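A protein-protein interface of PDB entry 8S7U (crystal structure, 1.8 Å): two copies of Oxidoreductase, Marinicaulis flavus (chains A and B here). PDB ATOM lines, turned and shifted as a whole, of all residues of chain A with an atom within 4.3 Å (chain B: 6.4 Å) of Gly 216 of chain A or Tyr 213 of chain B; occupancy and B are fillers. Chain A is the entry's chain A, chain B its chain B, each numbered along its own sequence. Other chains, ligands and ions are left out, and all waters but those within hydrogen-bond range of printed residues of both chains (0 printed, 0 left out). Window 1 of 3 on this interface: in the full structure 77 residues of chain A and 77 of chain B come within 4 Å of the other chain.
The backbone NH (N) of Ile 217 of chain A is in hydrogen-bond range of the backbone carbonyl oxygen (O) of Tyr 213 of chain B, 3.2 Å away. O of Gly 216 of chain A lies within hydrogen-bond range of N of Tyr 213 of chain B, 3.0 Å away.
OG of Ser 219 of chain A sits at hydrogen-bond distance from O of Gly 216 of chain A (2.6 Å).
Tyr 208 of chain B touches Phe 174 of chain A (OH to CB, 3.6 Å). O of Ile 217 of chain A touches CB of Pro 212 of chain B, 3.8 Å away. Ile 217 of chain A touches Ile 217 of chain B (CG2 to CG2, 3.3 Å). Ser 219 of chain A touches Gly 211 of chain B (O to O, 3.8 Å). Ser 219 of chain A touches Pro 212 of chain B. OG of Ser 219 of chain A touches CB of Tyr 213 of chain B (3.7 Å).
Of the printed residues of chain A, Pro 212 of chain B touches Ile 217 (3.8 Å) and Ser 219 (3.3 Å). Of the printed residues of chain B, Phe 174 of chain A touches Tyr 208 (3.6 Å). Of the printed residues of chain A, Ile 217 of chain B touches Ile 217. Ala 175 of chain B touches none of the printed residues of chain A. Gln 177 of chain B touches none of the printed residues of chain A. The nearest printed residue of chain B that does not touch Phe 174 of chain A is Tyr 213 of chain B (4.2 Å).
Hydrophobic or aromatic side chains of chain A that line the printed part of chain B: Phe 174 and Ile 217. Hydrophobic or aromatic side chains of chain B within 4 Å of the printed part of chain A: Tyr 208, Pro 212, Tyr 213 and Ile 217. Among the printed residues, 8 pairs touch across the chains. Among the printed residues, no Asp or Glu carboxylate lies within 4 Å of a Lys or Arg side-chain nitrogen of the other chain.
Ile 217 of chain A touches its own counterpart, Ile 217 of chain B. Of the 8 pairs that touch across the chains among the printed residues, 1 has its exchanged pair printed and touching as well.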
ATOM      1  N   PHE A 174      27.089 -11.580  13.823  1.00  0.00           N
ATOM      2  CA  PHE A 174      25.937 -10.877  13.242  1.00  0.00           C
ATOM      3  C   PHE A 174      26.232 -10.445  11.808  1.00  0.00           C
ATOM      4  O   PHE A 174      25.306 -10.348  10.956  1.00  0.00           O
ATOM      5  CB  PHE A 174      25.474  -9.710  14.103  1.00  0.00           C
ATOM      6  CG  PHE A 174      24.101  -9.294  13.649  1.00  0.00           C
ATOM      7  CD1 PHE A 174      23.020 -10.126  13.844  1.00  0.00           C
ATOM      8  CD2 PHE A 174      23.916  -8.094  12.982  1.00  0.00           C
ATOM      9  CE1 PHE A 174      21.774  -9.794  13.344  1.00  0.00           C
ATOM     10  CE2 PHE A 174      22.665  -7.761  12.496  1.00  0.00           C
ATOM     11  CZ  PHE A 174      21.605  -8.607  12.670  1.00  0.00           C
ATOM     12  N   VAL A 214      16.413  -3.824   7.870  1.00  0.00           N
ATOM     13  CA  VAL A 214      15.962  -3.812   9.279  1.00  0.00           C
ATOM     14  C   VAL A 214      16.549  -4.922  10.127  1.00  0.00           C
ATOM     15  O   VAL A 214      16.232  -4.930  11.320  1.00  0.00           O
ATOM     16  CB  VAL A 214      14.422  -3.866   9.327  1.00  0.00           C
ATOM     17  CG1 VAL A 214      13.850  -2.627   8.666  1.00  0.00           C
ATOM     18  CG2 VAL A 214      13.879  -5.142   8.703  1.00  0.00           C
ATOM     19  N   ASP A 215      17.252  -5.889   9.532  1.00  0.00           N
ATOM     20  CA  ASP A 215      17.657  -7.080  10.301  1.00  0.00           C
ATOM     21  C   ASP A 215      18.340  -6.619  11.591  1.00  0.00           C
ATOM     22  O   ASP A 215      18.138  -7.226  12.615  1.00  0.00           O
ATOM     23  CB  ASP A 215      18.546  -8.015   9.477  1.00  0.00           C
ATOM     24  CG  ASP A 215      17.880  -8.584   8.234  1.00  0.00           C
ATOM     25  OD1 ASP A 215      17.429  -7.787   7.399  1.00  0.00           O
ATOM     26  OD2 ASP A 215      17.759  -9.847   8.151  1.00  0.00           O
ATOM     27  N   GLY A 216      19.257  -5.664  11.510  1.00  0.00           N
ATOM     28  CA  GLY A 216      20.052  -5.228  12.657  1.00  0.00           C
ATOM     29  C   GLY A 216      19.192  -4.694  13.803  1.00  0.00           C
ATOM     30  O   GLY A 216      19.664  -4.808  14.988  1.00  0.00           O
ATOM     31  N   ILE A 217      17.978  -4.205  13.541  1.00  0.00           N
ATOM     32  CA  ILE A 217      17.161  -3.602  14.642  1.00  0.00           C
ATOM     33  C   ILE A 217      16.617  -4.709  15.545  1.00  0.00           C
ATOM     34  O   ILE A 217      16.235  -4.397  16.682  1.00  0.00           O
ATOM     35  CB  ILE A 217      16.017  -2.696  14.180  1.00  0.00           C
ATOM     36  CG1 ILE A 217      14.772  -3.486  13.793  1.00  0.00           C
ATOM     37  CG2 ILE A 217      16.503  -1.747  13.090  1.00  0.00           C
ATOM     38  CD1 ILE A 217      13.571  -2.667  13.490  1.00  0.00           C
ATOM     39  N   PHE A 218      16.787  -5.971  15.172  1.00  0.00           N
ATOM     40  CA  PHE A 218      16.317  -7.107  16.046  1.00  0.00           C
ATOM     41  C   PHE A 218      17.499  -7.708  16.815  1.00  0.00           C
ATOM     42  O   PHE A 218      17.319  -8.716  17.536  1.00  0.00           O
ATOM     43  CB  PHE A 218      15.630  -8.144  15.175  1.00  0.00           C
ATOM     44  CG  PHE A 218      14.376  -7.565  14.551  1.00  0.00           C
ATOM     45  CD1 PHE A 218      13.303  -7.134  15.329  1.00  0.00           C
ATOM     46  CD2 PHE A 218      14.320  -7.290  13.191  1.00  0.00           C
ATOM     47  CE1 PHE A 218      12.184  -6.565  14.747  1.00  0.00           C
ATOM     48  CE2 PHE A 218      13.189  -6.754  12.617  1.00  0.00           C
ATOM     49  CZ  PHE A 218      12.135  -6.347  13.392  1.00  0.00           C
ATOM     50  N   SER A 219      18.709  -7.151  16.637  1.00  0.00           N
ATOM     51  CA  SER A 219      19.915  -7.543  17.405  1.00  0.00           C
ATOM     52  C   SER A 219      20.077  -6.620  18.616  1.00  0.00           C
ATOM     53  O   SER A 219      19.733  -5.416  18.550  1.00  0.00           O
ATOM     54  CB  SER A 219      21.123  -7.581  16.490  1.00  0.00           C
ATOM     55  OG  SER A 219      21.535  -6.254  16.081  1.00  0.00           O
ATOM     56  N   PHE B 174      27.056  -0.200   0.819  1.00  0.00           N
ATOM     57  CA  PHE B 174      26.405  -0.057   2.129  1.00  0.00           C
ATOM     58  C   PHE B 174      27.091  -0.963   3.139  1.00  0.00           C
ATOM     59  O   PHE B 174      27.140  -0.616   4.350  1.00  0.00           O
ATOM     60  CB  PHE B 174      24.901  -0.292   2.118  1.00  0.00           C
ATOM     61  CG  PHE B 174      24.300   0.220   3.404  1.00  0.00           C
ATOM     62  CD1 PHE B 174      24.277   1.594   3.665  1.00  0.00           C
ATOM     63  CD2 PHE B 174      23.771  -0.637   4.354  1.00  0.00           C
ATOM     64  CE1 PHE B 174      23.849   2.086   4.883  1.00  0.00           C
ATOM     65  CE2 PHE B 174      23.341  -0.137   5.580  1.00  0.00           C
ATOM     66  CZ  PHE B 174      23.358   1.221   5.836  1.00  0.00           C
ATOM     67  N   ALA B 175      27.616  -2.129   2.744  1.00  0.00           N
ATOM     68  CA  ALA B 175      28.235  -3.050   3.730  1.00  0.00           C
ATOM     69  C   ALA B 175      29.487  -2.383   4.311  1.00  0.00           C
ATOM     70  O   ALA B 175      29.906  -2.745   5.413  1.00  0.00           O
ATOM     71  CB  ALA B 175      28.608  -4.400   3.068  1.00  0.00           C
ATOM     72  N   GLN B 177      29.784   0.737   5.088  1.00  0.00           N
ATOM     73  CA  GLN B 177      29.358   1.918   5.906  1.00  0.00           C
ATOM     74  C   GLN B 177      29.699   1.675   7.361  1.00  0.00           C
ATOM     75  O   GLN B 177      29.600   0.516   7.879  1.00  0.00           O
ATOM     76  CB  GLN B 177      27.887   2.239   5.639  1.00  0.00           C
ATOM     77  CG  GLN B 177      27.328   3.383   6.481  1.00  0.00           C
ATOM     78  CD  GLN B 177      26.742   2.899   7.782  1.00  0.00           C
ATOM     79  OE1 GLN B 177      26.316   1.745   7.893  1.00  0.00           O
ATOM     80  NE2 GLN B 177      26.669   3.780   8.785  1.00  0.00           N
ATOM     81  N   CYS B 178      30.124   2.711   8.083  1.00  0.00           N
ATOM     82  CA  CYS B 178      30.371   2.597   9.542  1.00  0.00           C
ATOM     83  C   CYS B 178      30.118   3.958  10.208  1.00  0.00           C
ATOM     84  O   CYS B 178      30.961   4.863  10.028  1.00  0.00           O
ATOM     85  CB  CYS B 178      31.777   2.088   9.798  1.00  0.00           C
ATOM     86  SG  CYS B 178      32.145   1.706  11.513  1.00  0.00           S
ATOM     87  N   LYS B 207      31.085  -0.772  13.898  1.00  0.00           N
ATOM     88  CA  LYS B 207      29.734  -0.474  13.306  1.00  0.00           C
ATOM     89  C   LYS B 207      28.667  -0.390  14.403  1.00  0.00           C
ATOM     90  O   LYS B 207      27.785   0.487  14.370  1.00  0.00           O
ATOM     91  CB  LYS B 207      29.358  -1.542  12.286  1.00  0.00           C
ATOM     92  CG  LYS B 207      30.120  -1.491  10.991  1.00  0.00           C
ATOM     93  CD  LYS B 207      30.035  -2.823  10.264  1.00  0.00           C
ATOM     94  CE  LYS B 207      30.238  -2.718   8.765  1.00  0.00           C
ATOM     95  NZ  LYS B 207      29.084  -2.078   8.078  1.00  0.00           N
ATOM     96  N   TYR B 208      28.608  -1.357  15.318  1.00  0.00           N
ATOM     97  CA  TYR B 208      27.360  -1.589  16.073  1.00  0.00           C
ATOM     98  C   TYR B 208      27.121  -0.529  17.146  1.00  0.00           C
ATOM     99  O   TYR B 208      25.996  -0.162  17.330  1.00  0.00           O
ATOM    100  CB  TYR B 208      27.303  -2.984  16.686  1.00  0.00           C
ATOM    101  CG  TYR B 208      27.478  -4.126  15.715  1.00  0.00           C
ATOM    102  CD1 TYR B 208      26.903  -4.121  14.454  1.00  0.00           C
ATOM    103  CD2 TYR B 208      28.190  -5.258  16.094  1.00  0.00           C
ATOM    104  CE1 TYR B 208      27.084  -5.182  13.559  1.00  0.00           C
ATOM    105  CE2 TYR B 208      28.340  -6.334  15.228  1.00  0.00           C
ATOM    106  CZ  TYR B 208      27.766  -6.315  13.973  1.00  0.00           C
ATOM    107  OH  TYR B 208      28.021  -7.339  13.101  1.00  0.00           O
ATOM    108  N   GLY B 209      28.138  -0.123  17.872  1.00  0.00           N
ATOM    109  CA  GLY B 209      27.934   0.471  19.197  1.00  0.00           C
ATOM    110  C   GLY B 209      27.240  -0.521  20.098  1.00  0.00           C
ATOM    111  O   GLY B 209      27.708  -1.711  20.181  1.00  0.00           O
ATOM    112  N   TYR B 210      26.169  -0.078  20.730  1.00  0.00           N
ATOM    113  CA  TYR B 210      25.415  -0.871  21.717  1.00  0.00           C
ATOM    114  C   TYR B 210      23.922  -0.747  21.421  1.00  0.00           C
ATOM    115  O   TYR B 210      23.486   0.324  21.048  1.00  0.00           O
ATOM    116  CB  TYR B 210      25.779  -0.398  23.120  1.00  0.00           C
ATOM    117  CG  TYR B 210      24.884  -0.879  24.239  1.00  0.00           C
ATOM    118  CD1 TYR B 210      24.981  -2.164  24.751  1.00  0.00           C
ATOM    119  CD2 TYR B 210      24.033  -0.005  24.873  1.00  0.00           C
ATOM    120  CE1 TYR B 210      24.185  -2.589  25.811  1.00  0.00           C
ATOM    121  CE2 TYR B 210      23.234  -0.412  25.926  1.00  0.00           C
ATOM    122  CZ  TYR B 210      23.340  -1.696  26.429  1.00  0.00           C
ATOM    123  OH  TYR B 210      22.578  -2.029  27.530  1.00  0.00           O
ATOM    124  N   GLY B 211      23.167  -1.836  21.626  1.00  0.00           N
ATOM    125  CA  GLY B 211      21.721  -1.811  21.394  1.00  0.00           C
ATOM    126  C   GLY B 211      21.399  -2.087  19.940  1.00  0.00           C
ATOM    127  O   GLY B 211      22.205  -2.586  19.129  1.00  0.00           O
ATOM    128  N   PRO B 212      20.139  -1.797  19.544  1.00  0.00           N
ATOM    129  CA  PRO B 212      19.695  -2.128  18.211  1.00  0.00           C
ATOM    130  C   PRO B 212      20.595  -1.484  17.143  1.00  0.00           C
ATOM    131  O   PRO B 212      20.979  -0.310  17.239  1.00  0.00           O
ATOM    132  CB  PRO B 212      18.253  -1.605  18.183  1.00  0.00           C
ATOM    133  CG  PRO B 212      17.822  -1.540  19.640  1.00  0.00           C
ATOM    134  CD  PRO B 212      19.089  -1.222  20.389  1.00  0.00           C
ATOM    135  N   TYR B 213      20.854  -2.257  16.094  1.00  0.00           N
ATOM    136  CA  TYR B 213      21.734  -1.841  14.992  1.00  0.00           C
ATOM    137  C   TYR B 213      20.819  -1.265  13.914  1.00  0.00           C
ATOM    138  O   TYR B 213      20.224  -2.022  13.156  1.00  0.00           O
ATOM    139  CB  TYR B 213      22.568  -3.048  14.548  1.00  0.00           C
ATOM    140  CG  TYR B 213      23.550  -2.778  13.434  1.00  0.00           C
ATOM    141  CD1 TYR B 213      24.144  -1.524  13.276  1.00  0.00           C
ATOM    142  CD2 TYR B 213      23.858  -3.762  12.481  1.00  0.00           C
ATOM    143  CE1 TYR B 213      25.054  -1.270  12.258  1.00  0.00           C
ATOM    144  CE2 TYR B 213      24.748  -3.517  11.454  1.00  0.00           C
ATOM    145  CZ  TYR B 213      25.352  -2.267  11.337  1.00  0.00           C
ATOM    146  OH  TYR B 213      26.253  -2.045  10.337  1.00  0.00           O
ATOM    147  N   VAL B 214      20.687   0.060  13.887  1.00  0.00           N
ATOM    148  CA  VAL B 214      19.668   0.790  13.087  1.00  0.00           C
ATOM    149  C   VAL B 214      20.216   1.420  11.823  1.00  0.00           C
ATOM    150  O   VAL B 214      19.373   1.894  11.039  1.00  0.00           O
ATOM    151  CB  VAL B 214      18.992   1.868  13.935  1.00  0.00           C
ATOM    152  CG1 VAL B 214      18.338   1.225  15.140  1.00  0.00           C
ATOM    153  CG2 VAL B 214      19.958   2.966  14.349  1.00  0.00           C
ATOM    154  N   ASP B 215      21.531   1.406  11.554  1.00  0.00           N
ATOM    155  CA  ASP B 215      22.015   2.157  10.365  1.00  0.00           C
ATOM    156  C   ASP B 215      21.230   1.762   9.098  1.00  0.00           C
ATOM    157  O   ASP B 215      20.908   2.641   8.275  1.00  0.00           O
ATOM    158  CB  ASP B 215      23.524   1.940  10.166  1.00  0.00           C
ATOM    159  CG  ASP B 215      24.353   2.468  11.339  1.00  0.00           C
ATOM    160  OD1 ASP B 215      24.143   1.996  12.435  1.00  0.00           O
ATOM    161  OD2 ASP B 215      25.192   3.355  11.143  1.00  0.00           O
ATOM    162  N   GLY B 216      21.028   0.458   8.871  1.00  0.00           N
ATOM    163  CA  GLY B 216      20.411  -0.053   7.642  1.00  0.00           C
ATOM    164  C   GLY B 216      18.966   0.445   7.469  1.00  0.00           C
ATOM    165  O   GLY B 216      18.518   0.551   6.299  1.00  0.00           O
ATOM    166  N   ILE B 217      18.293   0.907   8.527  1.00  0.00           N
ATOM    167  CA  ILE B 217      16.877   1.394   8.365  1.00  0.00           C
ATOM    168  C   ILE B 217      16.863   2.742   7.637  1.00  0.00           C
ATOM    169  O   ILE B 217      15.777   3.096   7.112  1.00  0.00           O
ATOM    170  CB  ILE B 217      16.048   1.455   9.654  1.00  0.00           C
ATOM    171  CG1 ILE B 217      16.289   2.708  10.490  1.00  0.00           C
ATOM    172  CG2 ILE B 217      16.218   0.174  10.454  1.00  0.00           C
ATOM    173  CD1 ILE B 217      15.372   2.808  11.695  1.00  0.00           C
